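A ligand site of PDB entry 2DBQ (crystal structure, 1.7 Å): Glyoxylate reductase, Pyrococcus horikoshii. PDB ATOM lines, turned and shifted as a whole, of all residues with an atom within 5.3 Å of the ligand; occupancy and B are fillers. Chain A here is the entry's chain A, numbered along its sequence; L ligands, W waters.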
ATOM      1  N   VAL A  76      12.877  -4.587   9.284  1.00  0.00           N
ATOM      2  CA  VAL A  76      11.926  -4.339  10.370  1.00  0.00           C
ATOM      3  C   VAL A  76      12.657  -4.566  11.700  1.00  0.00           C
ATOM      4  O   VAL A  76      12.334  -3.931  12.697  1.00  0.00           O
ATOM      5  CB  VAL A  76      10.669  -5.253  10.273  1.00  0.00           C
ATOM      6  CG1 VAL A  76      11.047  -6.695  10.282  1.00  0.00           C
ATOM      7  CG2 VAL A  76       9.721  -4.938  11.425  1.00  0.00           C
ATOM      8  N   GLY A  77      13.647  -5.451  11.691  1.00  0.00           N
ATOM      9  CA  GLY A  77      14.412  -5.674  12.898  1.00  0.00           C
ATOM     10  C   GLY A  77      15.412  -4.539  13.061  1.00  0.00           C
ATOM     11  O   GLY A  77      15.747  -3.846  12.095  1.00  0.00           O
ATOM     12  N   ASP A  79      18.179  -4.956  15.704  1.00  0.00           N
ATOM     13  CA  ASP A  79      19.144  -5.447  16.667  1.00  0.00           C
ATOM     14  C   ASP A  79      20.564  -5.022  16.260  1.00  0.00           C
ATOM     15  O   ASP A  79      21.529  -5.238  16.992  1.00  0.00           O
ATOM     16  CB  ASP A  79      19.045  -6.970  16.794  1.00  0.00           C
ATOM     17  CG  ASP A  79      18.969  -7.680  15.447  1.00  0.00           C
ATOM     18  OD1 ASP A  79      17.935  -7.542  14.754  1.00  0.00           O
ATOM     19  OD2 ASP A  79      19.939  -8.377  15.086  1.00  0.00           O
ATOM     20  N   PRO A  97       8.369  -1.838   9.230  1.00  0.00           N
ATOM     21  CA  PRO A  97       7.371  -2.842   9.626  1.00  0.00           C
ATOM     22  C   PRO A  97       6.189  -2.838   8.651  1.00  0.00           C
ATOM     23  O   PRO A  97       6.023  -1.900   7.859  1.00  0.00           O
ATOM     24  CB  PRO A  97       6.958  -2.366  11.018  1.00  0.00           C
ATOM     25  CG  PRO A  97       7.006  -0.876  10.872  1.00  0.00           C
ATOM     26  CD  PRO A  97       8.338  -0.684  10.139  1.00  0.00           C
ATOM     27  N   LEU A 100       6.658  -5.609   4.767  1.00  0.00           N
ATOM     28  CA  LEU A 100       7.302  -6.886   4.461  1.00  0.00           C
ATOM     29  C   LEU A 100       6.641  -8.042   5.217  1.00  0.00           C
ATOM     30  O   LEU A 100       7.124  -9.171   5.186  1.00  0.00           O
ATOM     31  CB  LEU A 100       8.799  -6.820   4.820  1.00  0.00           C
ATOM     32  CG  LEU A 100       9.231  -6.197   6.151  1.00  0.00           C
ATOM     33  CD1 LEU A 100       8.510  -6.844   7.334  1.00  0.00           C
ATOM     34  CD2 LEU A 100      10.735  -6.350   6.307  1.00  0.00           C
ATOM     35  N   THR A 104       7.321 -12.176   4.338  1.00  0.00           N
ATOM     36  CA  THR A 104       7.973 -13.000   5.341  1.00  0.00           C
ATOM     37  C   THR A 104       7.073 -14.136   5.823  1.00  0.00           C
ATOM     38  O   THR A 104       7.537 -15.255   6.038  1.00  0.00           O
ATOM     39  CB  THR A 104       8.437 -12.149   6.544  1.00  0.00           C
ATOM     40  OG1 THR A 104       9.137 -10.989   6.076  1.00  0.00           O
ATOM     41  CG2 THR A 104       9.385 -12.947   7.445  1.00  0.00           C
ATOM     42  N   ILE A 156       5.785 -18.629  18.209  1.00  0.00           N
ATOM     43  CA  ILE A 156       6.458 -17.933  19.303  1.00  0.00           C
ATOM     44  C   ILE A 156       6.721 -16.518  18.806  1.00  0.00           C
ATOM     45  O   ILE A 156       7.561 -16.297  17.923  1.00  0.00           O
ATOM     46  CB  ILE A 156       7.776 -18.655  19.672  1.00  0.00           C
ATOM     47  CG1 ILE A 156       7.454 -20.067  20.159  1.00  0.00           C
ATOM     48  CG2 ILE A 156       8.511 -17.870  20.761  1.00  0.00           C
ATOM     49  CD1 ILE A 156       8.666 -20.926  20.459  1.00  0.00           C
ATOM     50  N   GLY A 157       5.975 -15.569  19.360  1.00  0.00           N
ATOM     51  CA  GLY A 157       6.081 -14.187  18.954  1.00  0.00           C
ATOM     52  C   GLY A 157       4.870 -13.881  18.105  1.00  0.00           C
ATOM     53  O   GLY A 157       4.891 -14.096  16.894  1.00  0.00           O
ATOM     54  N   LEU A 158       3.780 -13.419  18.730  1.00  0.00           N
ATOM     55  CA  LEU A 158       2.559 -13.136  17.997  1.00  0.00           C
ATOM     56  C   LEU A 158       2.451 -11.659  17.623  1.00  0.00           C
ATOM     57  O   LEU A 158       1.495 -10.972  18.002  1.00  0.00           O
ATOM     58  CB  LEU A 158       1.329 -13.554  18.826  1.00  0.00           C
ATOM     59  CG  LEU A 158      -0.016 -13.636  18.070  1.00  0.00           C
ATOM     60  CD1 LEU A 158      -0.004 -14.819  17.107  1.00  0.00           C
ATOM     61  CD2 LEU A 158      -1.149 -13.786  19.064  1.00  0.00           C
ATOM     62  N   GLY A 159       3.429 -11.184  16.846  1.00  0.00           N
ATOM     63  CA  GLY A 159       3.427  -9.801  16.419  1.00  0.00           C
ATOM     64  C   GLY A 159       2.871  -9.659  15.007  1.00  0.00           C
ATOM     65  O   GLY A 159       1.966 -10.406  14.614  1.00  0.00           O
ATOM     66  N   ARG A 160       3.407  -8.704  14.252  1.00  0.00           N
ATOM     67  CA  ARG A 160       2.950  -8.492  12.889  1.00  0.00           C
ATOM     68  C   ARG A 160       3.076  -9.744  12.029  1.00  0.00           C
ATOM     69  O   ARG A 160       2.112 -10.165  11.379  1.00  0.00           O
ATOM     70  CB  ARG A 160       3.735  -7.330  12.255  1.00  0.00           C
ATOM     71  CG  ARG A 160       3.394  -5.968  12.851  1.00  0.00           C
ATOM     72  CD  ARG A 160       4.340  -4.878  12.357  1.00  0.00           C
ATOM     73  NE  ARG A 160       5.694  -5.087  12.830  1.00  0.00           N
ATOM     74  CZ  ARG A 160       6.336  -4.291  13.684  1.00  0.00           C
ATOM     75  NH1 ARG A 160       5.736  -3.205  14.171  1.00  0.00           N
ATOM     76  NH2 ARG A 160       7.579  -4.580  14.051  1.00  0.00           N
ATOM     77  N   ILE A 161       4.255 -10.347  12.027  1.00  0.00           N
ATOM     78  CA  ILE A 161       4.481 -11.537  11.228  1.00  0.00           C
ATOM     79  C   ILE A 161       3.869 -12.785  11.867  1.00  0.00           C
ATOM     80  O   ILE A 161       3.342 -13.638  11.169  1.00  0.00           O
ATOM     81  CB  ILE A 161       5.989 -11.716  10.960  1.00  0.00           C
ATOM     82  CG1 ILE A 161       6.460 -10.552  10.074  1.00  0.00           C
ATOM     83  CG2 ILE A 161       6.267 -13.066  10.302  1.00  0.00           C
ATOM     84  CD1 ILE A 161       7.939 -10.509   9.823  1.00  0.00           C
ATOM     85  N   GLY A 162       3.939 -12.875  13.188  1.00  0.00           N
ATOM     86  CA  GLY A 162       3.360 -14.014  13.876  1.00  0.00           C
ATOM     87  C   GLY A 162       1.864 -14.132  13.567  1.00  0.00           C
ATOM     88  O   GLY A 162       1.349 -15.233  13.321  1.00  0.00           O
ATOM     89  N   TYR A 179       2.822 -18.312  22.057  1.00  0.00           N
ATOM     90  CA  TYR A 179       3.457 -17.853  23.272  1.00  0.00           C
ATOM     91  C   TYR A 179       4.069 -16.534  22.842  1.00  0.00           C
ATOM     92  O   TYR A 179       4.794 -16.491  21.843  1.00  0.00           O
ATOM     93  CB  TYR A 179       4.570 -18.799  23.722  1.00  0.00           C
ATOM     94  CG  TYR A 179       5.410 -18.200  24.814  1.00  0.00           C
ATOM     95  CD1 TYR A 179       4.873 -17.962  26.091  1.00  0.00           C
ATOM     96  CD2 TYR A 179       6.724 -17.803  24.574  1.00  0.00           C
ATOM     97  CE1 TYR A 179       5.625 -17.352  27.087  1.00  0.00           C
ATOM     98  CE2 TYR A 179       7.499 -17.198  25.572  1.00  0.00           C
ATOM     99  CZ  TYR A 179       6.936 -16.979  26.829  1.00  0.00           C
ATOM    100  OH  TYR A 179       7.685 -16.370  27.816  1.00  0.00           O
ATOM    101  N   SER A 180       3.763 -15.468  23.570  1.00  0.00           N
ATOM    102  CA  SER A 180       4.307 -14.152  23.233  1.00  0.00           C
ATOM    103  C   SER A 180       4.404 -13.297  24.498  1.00  0.00           C
ATOM    104  O   SER A 180       3.827 -13.634  25.539  1.00  0.00           O
ATOM    105  CB  SER A 180       3.404 -13.471  22.198  1.00  0.00           C
ATOM    106  OG  SER A 180       4.061 -12.377  21.583  1.00  0.00           O
ATOM    107  N   ARG A 181       5.150 -12.200  24.400  1.00  0.00           N
ATOM    108  CA  ARG A 181       5.348 -11.298  25.531  1.00  0.00           C
ATOM    109  C   ARG A 181       4.054 -10.604  25.927  1.00  0.00           C
ATOM    110  O   ARG A 181       3.824 -10.310  27.105  1.00  0.00           O
ATOM    111  CB  ARG A 181       6.421 -10.282  25.179  1.00  0.00           C
ATOM    112  CG  ARG A 181       6.805  -9.346  26.295  1.00  0.00           C
ATOM    113  CD  ARG A 181       8.034  -8.541  25.895  1.00  0.00           C
ATOM    114  NE  ARG A 181       7.814  -7.763  24.678  1.00  0.00           N
ATOM    115  CZ  ARG A 181       8.748  -7.046  24.073  1.00  0.00           C
ATOM    116  NH1 ARG A 181       9.976  -7.003  24.577  1.00  0.00           N
ATOM    117  NH2 ARG A 181       8.463  -6.359  22.981  1.00  0.00           N
ATOM    118  N   THR A 182       3.204 -10.330  24.934  1.00  0.00           N
ATOM    119  CA  THR A 182       1.922  -9.679  25.158  1.00  0.00           C
ATOM    120  C   THR A 182       0.776 -10.575  24.675  1.00  0.00           C
ATOM    121  O   THR A 182       0.807 -11.080  23.552  1.00  0.00           O
ATOM    122  CB  THR A 182       1.840  -8.324  24.386  1.00  0.00           C
ATOM    123  OG1 THR A 182       2.740  -7.389  24.986  1.00  0.00           O
ATOM    124  CG2 THR A 182       0.419  -7.762  24.438  1.00  0.00           C
ATOM    125  N   LYS A 184      -2.867 -11.322  23.280  1.00  0.00           N
ATOM    126  CA  LYS A 184      -3.804 -10.611  22.430  1.00  0.00           C
ATOM    127  C   LYS A 184      -5.104 -11.413  22.357  1.00  0.00           C
ATOM    128  O   LYS A 184      -5.306 -12.209  21.454  1.00  0.00           O
ATOM    129  CB  LYS A 184      -3.181 -10.429  21.052  1.00  0.00           C
ATOM    130  CG  LYS A 184      -1.812  -9.753  21.157  1.00  0.00           C
ATOM    131  CD  LYS A 184      -1.201  -9.421  19.819  1.00  0.00           C
ATOM    132  CE  LYS A 184       0.131  -8.693  20.019  1.00  0.00           C
ATOM    133  NZ  LYS A 184       0.727  -8.275  18.710  1.00  0.00           N
ATOM    134  N   ALA A 211       9.018 -16.091  15.495  1.00  0.00           N
ATOM    135  CA  ALA A 211       8.769 -14.789  14.896  1.00  0.00           C
ATOM    136  C   ALA A 211       8.950 -13.672  15.930  1.00  0.00           C
ATOM    137  O   ALA A 211       8.145 -12.737  15.998  1.00  0.00           O
ATOM    138  CB  ALA A 211       7.361 -14.727  14.322  1.00  0.00           C
ATOM    139  N   VAL A 212      10.015 -13.785  16.717  1.00  0.00           N
ATOM    140  CA  VAL A 212      10.342 -12.783  17.738  1.00  0.00           C
ATOM    141  C   VAL A 212      11.606 -12.031  17.331  1.00  0.00           C
ATOM    142  O   VAL A 212      12.428 -12.539  16.571  1.00  0.00           O
ATOM    143  CB  VAL A 212      10.617 -13.427  19.134  1.00  0.00           C
ATOM    144  CG1 VAL A 212       9.350 -14.066  19.702  1.00  0.00           C
ATOM    145  CG2 VAL A 212      11.738 -14.452  19.035  1.00  0.00           C
ATOM    146  N   PRO A 213      11.777 -10.802  17.833  1.00  0.00           N
ATOM    147  CA  PRO A 213      12.991 -10.057  17.480  1.00  0.00           C
ATOM    148  C   PRO A 213      14.151 -10.581  18.335  1.00  0.00           C
ATOM    149  O   PRO A 213      13.914 -11.349  19.270  1.00  0.00           O
ATOM    150  CB  PRO A 213      12.618  -8.609  17.816  1.00  0.00           C
ATOM    151  CG  PRO A 213      11.650  -8.767  18.962  1.00  0.00           C
ATOM    152  CD  PRO A 213      10.812  -9.948  18.553  1.00  0.00           C
ATOM    153  N   LEU A 214      15.381 -10.214  18.013  1.00  0.00           N
ATOM    154  CA  LEU A 214      16.515 -10.659  18.814  1.00  0.00           C
ATOM    155  C   LEU A 214      16.769  -9.656  19.941  1.00  0.00           C
ATOM    156  O   LEU A 214      17.026  -8.479  19.685  1.00  0.00           O
ATOM    157  CB  LEU A 214      17.781 -10.796  17.965  1.00  0.00           C
ATOM    158  CG  LEU A 214      19.076 -11.077  18.745  1.00  0.00           C
ATOM    159  CD1 LEU A 214      18.965 -12.415  19.463  1.00  0.00           C
ATOM    160  CD2 LEU A 214      20.283 -11.060  17.803  1.00  0.00           C
ATOM    161  N   THR A 215      16.675 -10.126  21.172  1.00  0.00           N
ATOM    162  CA  THR A 215      16.922  -9.290  22.345  1.00  0.00           C
ATOM    163  C   THR A 215      17.696 -10.146  23.346  1.00  0.00           C
ATOM    164  O   THR A 215      18.001 -11.298  23.065  1.00  0.00           O
ATOM    165  CB  THR A 215      15.617  -8.815  23.014  1.00  0.00           C
ATOM    166  OG1 THR A 215      14.920  -9.933  23.573  1.00  0.00           O
ATOM    167  CG2 THR A 215      14.704  -8.126  22.004  1.00  0.00           C
ATOM    168  N   GLU A 217      16.562 -11.251  26.008  1.00  0.00           N
ATOM    169  CA  GLU A 217      15.596 -12.251  26.455  1.00  0.00           C
ATOM    170  C   GLU A 217      15.294 -13.370  25.461  1.00  0.00           C
ATOM    171  O   GLU A 217      14.891 -14.466  25.853  1.00  0.00           O
ATOM    172  CB  GLU A 217      14.287 -11.564  26.848  1.00  0.00           C
ATOM    173  CG  GLU A 217      14.449 -10.432  27.877  1.00  0.00           C
ATOM    174  CD  GLU A 217      14.781  -9.066  27.250  1.00  0.00           C
ATOM    175  OE1 GLU A 217      15.868  -8.908  26.644  1.00  0.00           O
ATOM    176  OE2 GLU A 217      13.945  -8.143  27.365  1.00  0.00           O
ATOM    177  N   THR A 218      15.485 -13.099  24.162  1.00  0.00           N
ATOM    178  CA  THR A 218      15.211 -14.123  23.154  1.00  0.00           C
ATOM    179  C   THR A 218      16.469 -14.837  22.677  1.00  0.00           C
ATOM    180  O   THR A 218      16.387 -15.825  21.945  1.00  0.00           O
ATOM    181  CB  THR A 218      14.482 -13.535  21.919  1.00  0.00           C
ATOM    182  OG1 THR A 218      15.304 -12.547  21.303  1.00  0.00           O
ATOM    183  CG2 THR A 218      13.162 -12.903  22.334  1.00  0.00           C
ATOM    184  N   ILE A 239      12.329 -17.801  11.063  1.00  0.00           N
ATOM    185  CA  ILE A 239      12.408 -16.690  10.105  1.00  0.00           C
ATOM    186  C   ILE A 239      12.652 -15.415  10.886  1.00  0.00           C
ATOM    187  O   ILE A 239      12.567 -14.312  10.344  1.00  0.00           O
ATOM    188  CB  ILE A 239      11.102 -16.520   9.247  1.00  0.00           C
ATOM    189  CG1 ILE A 239       9.857 -16.392  10.131  1.00  0.00           C
ATOM    190  CG2 ILE A 239      10.966 -17.693   8.299  1.00  0.00           C
ATOM    191  CD1 ILE A 239       9.694 -15.038  10.796  1.00  0.00           C
ATOM    192  N   ALA A 240      12.964 -15.576  12.172  1.00  0.00           N
ATOM    193  CA  ALA A 240      13.216 -14.444  13.077  1.00  0.00           C
ATOM    194  C   ALA A 240      14.675 -13.993  12.999  1.00  0.00           C
ATOM    195  O   ALA A 240      15.044 -13.165  12.154  1.00  0.00           O
ATOM    196  CB  ALA A 240      12.861 -14.851  14.514  1.00  0.00           C
ATOM    197  N   ARG A 241      15.502 -14.518  13.892  1.00  0.00           N
ATOM    198  CA  ARG A 241      16.920 -14.219  13.937  1.00  0.00           C
ATOM    199  C   ARG A 241      17.660 -15.503  14.300  1.00  0.00           C
ATOM    200  O   ARG A 241      17.167 -16.311  15.095  1.00  0.00           O
ATOM    201  CB  ARG A 241      17.218 -13.130  14.981  1.00  0.00           C
ATOM    202  CG  ARG A 241      16.888 -11.721  14.522  1.00  0.00           C
ATOM    203  CD  ARG A 241      17.877 -11.233  13.456  1.00  0.00           C
ATOM    204  NE  ARG A 241      17.619  -9.842  13.089  1.00  0.00           N
ATOM    205  CZ  ARG A 241      16.814  -9.451  12.106  1.00  0.00           C
ATOM    206  NH1 ARG A 241      16.159 -10.326  11.355  1.00  0.00           N
ATOM    207  NH2 ARG A 241      16.648  -8.145  11.887  1.00  0.00           N
ATOM    208  N   ASP A 265      15.774 -19.529   7.787  1.00  0.00           N
ATOM    209  CA  ASP A 265      16.035 -18.415   6.863  1.00  0.00           C
ATOM    210  C   ASP A 265      17.071 -17.459   7.480  1.00  0.00           C
ATOM    211  O   ASP A 265      17.568 -16.547   6.812  1.00  0.00           O
ATOM    212  CB  ASP A 265      14.741 -17.633   6.595  1.00  0.00           C
ATOM    213  CG  ASP A 265      14.941 -16.517   5.565  1.00  0.00           C
ATOM    214  OD1 ASP A 265      15.397 -16.826   4.439  1.00  0.00           O
ATOM    215  OD2 ASP A 265      14.628 -15.347   5.869  1.00  0.00           O
ATOM    216  N   VAL A 266      17.386 -17.674   8.761  1.00  0.00           N
ATOM    217  CA  VAL A 266      18.330 -16.812   9.461  1.00  0.00           C
ATOM    218  C   VAL A 266      19.363 -17.629  10.242  1.00  0.00           C
ATOM    219  O   VAL A 266      19.071 -18.728  10.698  1.00  0.00           O
ATOM    220  CB  VAL A 266      17.583 -15.874  10.419  1.00  0.00           C
ATOM    221  CG1 VAL A 266      16.733 -14.898   9.618  1.00  0.00           C
ATOM    222  CG2 VAL A 266      16.706 -16.686  11.360  1.00  0.00           C
ATOM    223  N   HIS A 288      18.350 -15.576   4.322  1.00  0.00           N
ATOM    224  CA  HIS A 288      17.645 -14.392   4.796  1.00  0.00           C
ATOM    225  C   HIS A 288      16.896 -13.702   3.653  1.00  0.00           C
ATOM    226  O   HIS A 288      17.111 -12.521   3.370  1.00  0.00           O
ATOM    227  CB  HIS A 288      18.649 -13.422   5.435  1.00  0.00           C
ATOM    228  CG  HIS A 288      18.026 -12.486   6.430  1.00  0.00           C
ATOM    229  ND1 HIS A 288      18.680 -12.100   7.581  1.00  0.00           N
ATOM    230  CD2 HIS A 288      16.827 -11.863   6.448  1.00  0.00           C
ATOM    231  CE1 HIS A 288      17.899 -11.268   8.273  1.00  0.00           C
ATOM    232  NE2 HIS A 288      16.770 -11.110   7.604  1.00  0.00           N
ATOM    233  N   ILE A 289      16.023 -14.466   2.998  1.00  0.00           N
ATOM    234  CA  ILE A 289      15.222 -13.967   1.891  1.00  0.00           C
ATOM    235  C   ILE A 289      13.761 -13.766   2.300  1.00  0.00           C
ATOM    236  O   ILE A 289      12.882 -13.727   1.447  1.00  0.00           O
ATOM    237  CB  ILE A 289      15.273 -14.932   0.678  1.00  0.00           C
ATOM    238  CG1 ILE A 289      14.705 -16.304   1.064  1.00  0.00           C
ATOM    239  CG2 ILE A 289      16.707 -15.068   0.196  1.00  0.00           C
ATOM    240  CD1 ILE A 289      14.648 -17.292  -0.091  1.00  0.00           C
ATOM    241  N   GLY A 290      13.512 -13.652   3.595  1.00  0.00           N
ATOM    242  CA  GLY A 290      12.155 -13.461   4.082  1.00  0.00           C
ATOM    243  C   GLY A 290      11.378 -12.352   3.387  1.00  0.00           C
ATOM    244  O   GLY A 290      10.240 -12.555   2.975  1.00  0.00           O
ATOM    245  N   SER A 291      11.996 -11.181   3.234  1.00  0.00           N
ATOM    246  CA  SER A 291      11.323 -10.055   2.592  1.00  0.00           C
ATOM    247  C   SER A 291      11.717  -9.879   1.114  1.00  0.00           C
ATOM    248  O   SER A 291      11.482  -8.834   0.521  1.00  0.00           O
ATOM    249  CB  SER A 291      11.634  -8.760   3.354  1.00  0.00           C
ATOM    250  OG  SER A 291      13.026  -8.498   3.393  1.00  0.00           O
HETATM  251  P1  LIG L   1       6.811  -7.382  15.889  1.00  0.00           P
HETATM  252  O1  LIG L   1       5.422  -7.167  15.406  1.00  0.00           O
HETATM  253  O2  LIG L   1       7.415  -6.704  17.056  1.00  0.00           O
HETATM  254  O3  LIG L   1       6.579  -8.848  16.520  1.00  0.00           O
HETATM  255  C1  LIG L   1       7.466  -9.412  17.492  1.00  0.00           C
HETATM  256  C2  LIG L   1       6.707 -10.324  18.453  1.00  0.00           C
HETATM  257  O4  LIG L   1       7.662 -10.935  19.348  1.00  0.00           O
HETATM  258  C3  LIG L   1       5.736  -9.518  19.323  1.00  0.00           C
HETATM  259  O5  LIG L   1       4.567 -10.297  19.586  1.00  0.00           O
HETATM  260  C4  LIG L   1       6.549  -9.332  20.609  1.00  0.00           C
HETATM  261  O6  LIG L   1       5.672  -9.128  21.725  1.00  0.00           O
HETATM  262  C5  LIG L   1       7.155 -10.733  20.683  1.00  0.00           C
HETATM  263  N1  LIG L   1       8.249 -10.825  21.683  1.00  0.00           N
HETATM  264  C6  LIG L   1       9.240  -9.960  21.863  1.00  0.00           C
HETATM  265  N2  LIG L   1      10.020 -10.374  22.859  1.00  0.00           N
HETATM  266  C7  LIG L   1       9.519 -11.511  23.330  1.00  0.00           C
HETATM  267  C8  LIG L   1       9.871 -12.394  24.333  1.00  0.00           C
HETATM  268  N3  LIG L   1      10.932 -12.149  25.108  1.00  0.00           N
HETATM  269  N4  LIG L   1       9.130 -13.489  24.537  1.00  0.00           N
HETATM  270  C9  LIG L   1       8.067 -13.746  23.797  1.00  0.00           C
HETATM  271  N5  LIG L   1       7.696 -12.923  22.831  1.00  0.00           N
HETATM  272  C10 LIG L   1       8.389 -11.809  22.568  1.00  0.00           C
HETATM  273  O7  LIG L   1       7.926  -7.850  14.818  1.00  0.00           O
HETATM  274  P2  LIG L   1       7.591  -8.494  13.373  1.00  0.00           P
HETATM  275  O8  LIG L   1       6.509  -9.422  13.772  1.00  0.00           O
HETATM  276  O9  LIG L   1       7.397  -7.251  12.586  1.00  0.00           O
HETATM  277  O10 LIG L   1       9.076  -9.103  13.236  1.00  0.00           O
HETATM  278  C11 LIG L   1       9.645  -9.885  14.278  1.00  0.00           C
HETATM  279  C12 LIG L   1      11.101 -10.228  13.933  1.00  0.00           C
HETATM  280  O11 LIG L   1      11.158 -11.068  12.767  1.00  0.00           O
HETATM  281  C13 LIG L   1      11.878  -8.993  13.512  1.00  0.00           C
HETATM  282  O12 LIG L   1      12.314  -8.255  14.653  1.00  0.00           O
HETATM  283  C14 LIG L   1      13.070  -9.644  12.825  1.00  0.00           C
HETATM  284  O13 LIG L   1      14.058 -10.058  13.779  1.00  0.00           O
HETATM  285  C15 LIG L   1      12.445 -10.869  12.150  1.00  0.00           C
HETATM  286  N6  LIG L   1      12.212 -10.693  10.699  1.00  0.00           N
HETATM  287  C16 LIG L   1      12.900 -11.516   9.805  1.00  0.00           C
HETATM  288  C17 LIG L   1      12.667 -11.395   8.438  1.00  0.00           C
HETATM  289  C18 LIG L   1      13.433 -12.273   7.443  1.00  0.00           C
HETATM  290  O14 LIG L   1      13.725 -11.869   6.325  1.00  0.00           O
HETATM  291  N7  LIG L   1      13.783 -13.472   7.911  1.00  0.00           N
HETATM  292  C19 LIG L   1      11.759 -10.453   7.970  1.00  0.00           C
HETATM  293  C20 LIG L   1      11.056  -9.637   8.860  1.00  0.00           C
HETATM  294  C21 LIG L   1      11.289  -9.759  10.228  1.00  0.00           C
HETATM  295  P3  LIG L   1       5.044  -7.666  22.023  1.00  0.00           P
HETATM  296  O15 LIG L   1       3.470  -7.462  21.781  1.00  0.00           O
HETATM  297  O16 LIG L   1       6.054  -6.499  21.569  1.00  0.00           O
HETATM  298  O17 LIG L   1       5.138  -7.588  23.497  1.00  0.00           O
HETATM  299  O   HOH W   1      11.858  -5.644  15.070  1.00  0.00           O
HETATM  300  O   HOH W   2       9.808  -5.222  16.812  1.00  0.00           O
HETATM  301  O   HOH W   3       2.684 -10.407  21.861  1.00  0.00           O
HETATM  302  O   HOH W   4       3.213  -6.950  19.209  1.00  0.00           O
HETATM  303  O   HOH W   5      15.374  -8.316  15.705  1.00  0.00           O
HETATM  304  O   HOH W   6       3.298  -5.649  16.766  1.00  0.00           O
HETATM  305  O   HOH W   7       6.308  -6.366   9.958  1.00  0.00           O
HETATM  306  O   HOH W   8      13.754  -9.067   5.747  1.00  0.00           O
HETATM  307  O   HOH W   9       8.302  -6.618  19.805  1.00  0.00           O
HETATM  308  O   HOH W  10       5.741 -11.611  15.150  1.00  0.00           O
HETATM  309  O   HOH W  11       9.790 -15.338  26.779  1.00  0.00           O
HETATM  310  O   HOH W  12      12.324  -9.623  24.323  1.00  0.00           O
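The backbone NH (N) of Arg 160 sits at hydrogen-bond distance from an oxygen (O1) of the ligand.
The guanidinium group of Arg 160 lies within salt-bridge range of an oxygen (O9) of the ligand, at 2.8 Å.
The backbone NH (N) of Arg 181 is in hydrogen-bond range of a nitrogen (N5) of the ligand, at 3.1 Å.
O16 of the ligand lies within salt-bridge range of NH2 of Arg 181, at 2.8 Å.
The side-chain hydroxyl (OG1) of Thr 182 sits at hydrogen-bond distance from an oxygen (O17) of the ligand (2.8 Å).
A nitrogen (N7) of the ligand is in hydrogen-bond range of the backbone carbonyl oxygen of Ile 239.
The side-chain carboxylate of Asp 265 lies within hydrogen-bond range of a nitrogen (N7) of the ligand, at 2.9 Å.
An oxygen (O5) of the ligand lies within hydrogen-bond range of the side-chain hydroxyl of Ser 180, at 2.9 Å.
O8 of the ligand sits at hydrogen-bond distance from N of Ile 161, at 3.0 Å.
The backbone NH (N) of Gly 159 sits at hydrogen-bond distance from an oxygen (O5) of the ligand, 3.1 Å away.
A ring nitrogen (NE2) of His 288 sits close to an oxygen (O14) of the ligand.
The backbone NH of Gly 290 lies close to an oxygen (O14) of the ligand, 3.3 Å away.
N of Leu 158 sits close to O5 of the ligand (3.3 Å).
An oxygen (O13) of the ligand sits at hydrogen-bond distance from the guanidinium group (NH1) of Arg 241, at 3.2 Å.
The backbone carbonyl oxygen (O) of Asp 265 sits at hydrogen-bond distance from the backbone NH (N) of His 288 (2.8 Å).
O of Gly 290 sits at hydrogen-bond distance from N of Thr 104, at 3.2 Å.
The side-chain amino group (NZ) of Lys 184 is in hydrogen-bond range of the backbone carbonyl oxygen (O) of Leu 158, 2.9 Å away.
The backbone carbonyl oxygen (O) of Pro 213 is in hydrogen-bond range of the side-chain hydroxyl (OG1) of Thr 218, 2.7 Å away.
NE of Arg 241 lies within salt-bridge range of OD1 of Asp 79 (2.9 Å).
O of Tyr 179 is in hydrogen-bond range of N of Gly 157, 2.9 Å away.
O of Ile 156 lies within hydrogen-bond range of N of Ala 211, 2.8 Å away.
The backbone NH (N) of Glu 217 sits close to the side-chain hydroxyl (OG1) of Thr 215 (3.2 Å).
CG1 of Val 76 touches C21 of the ligand (3.1 Å).
Gly 77 touches the ligand (CA to O12, 3.8 Å).
Thr 104 touches the ligand.
Gly 157 touches the ligand.
CE2 of Tyr 179 touches C9 of the ligand (3.9 Å).
Lys 184 touches the ligand (CE to O15, 3.97 Å).
O of Ala 211 touches C11 of the ligand (3.7 Å).
Val 212 touches the ligand (CG1 to O4, 3.6 Å).
CB of Pro 213 touches O12 of the ligand (3.2 Å).
CB of Glu 217 touches N3 of the ligand, 3.8 Å away.
CG2 of Thr 218 touches N3 of the ligand, at 3.6 Å.
O of Ala 240 touches C15 of the ligand, at 3.5 Å.
Val 266 touches the ligand (CG1 to N7, 3.7 Å).
Ser 291 touches the ligand (N to O14, 3.6 Å).
Hydrophobic or aromatic side chains within 4 Å of the ligand: Val 76, Ile 161, Tyr 179, Val 212, Pro 213, Val 266 and His 288.
Of the 34 residues printed, 26 come within 4 Å of the ligand.
Along chain A the residues within 4 Å of the ligand span positions 76 to 291.
The nearest printed residue that does not touch the ligand is Leu 100 (4.1 Å).
Water W4 bridges an oxygen (O15) of the ligand (2.6 Å) and the side-chain amino group (NZ) of Lys 184 (2.9 Å).
Water W1 lies within hydrogen-bond range of an oxygen (O12) of the ligand and the backbone carbonyl oxygen of Val 76.
Water W10 lies within hydrogen-bond range of O8 of the ligand (2.7 Å), O of Ala 211 (2.8 Å), N of Gly 159 (2.9 Å), N of Gly 162 (2.9 Å) and O of Gly 157 (3.2 Å).
Water W9 lies within hydrogen-bond range of an oxygen (O16) of the ligand (2.9 Å) and the guanidinium group of Arg 181 (3.2 Å).
Water W5 lies within hydrogen-bond range of the side-chain carboxylate of Asp 79 (2.8 Å), an oxygen (O13) of the ligand (2.9 Å) and the backbone NH of Leu 214 (3.0 Å).
Water W7 lies within hydrogen-bond range of O9 of the ligand (3.0 Å) and NE of Arg 160 (3.2 Å).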
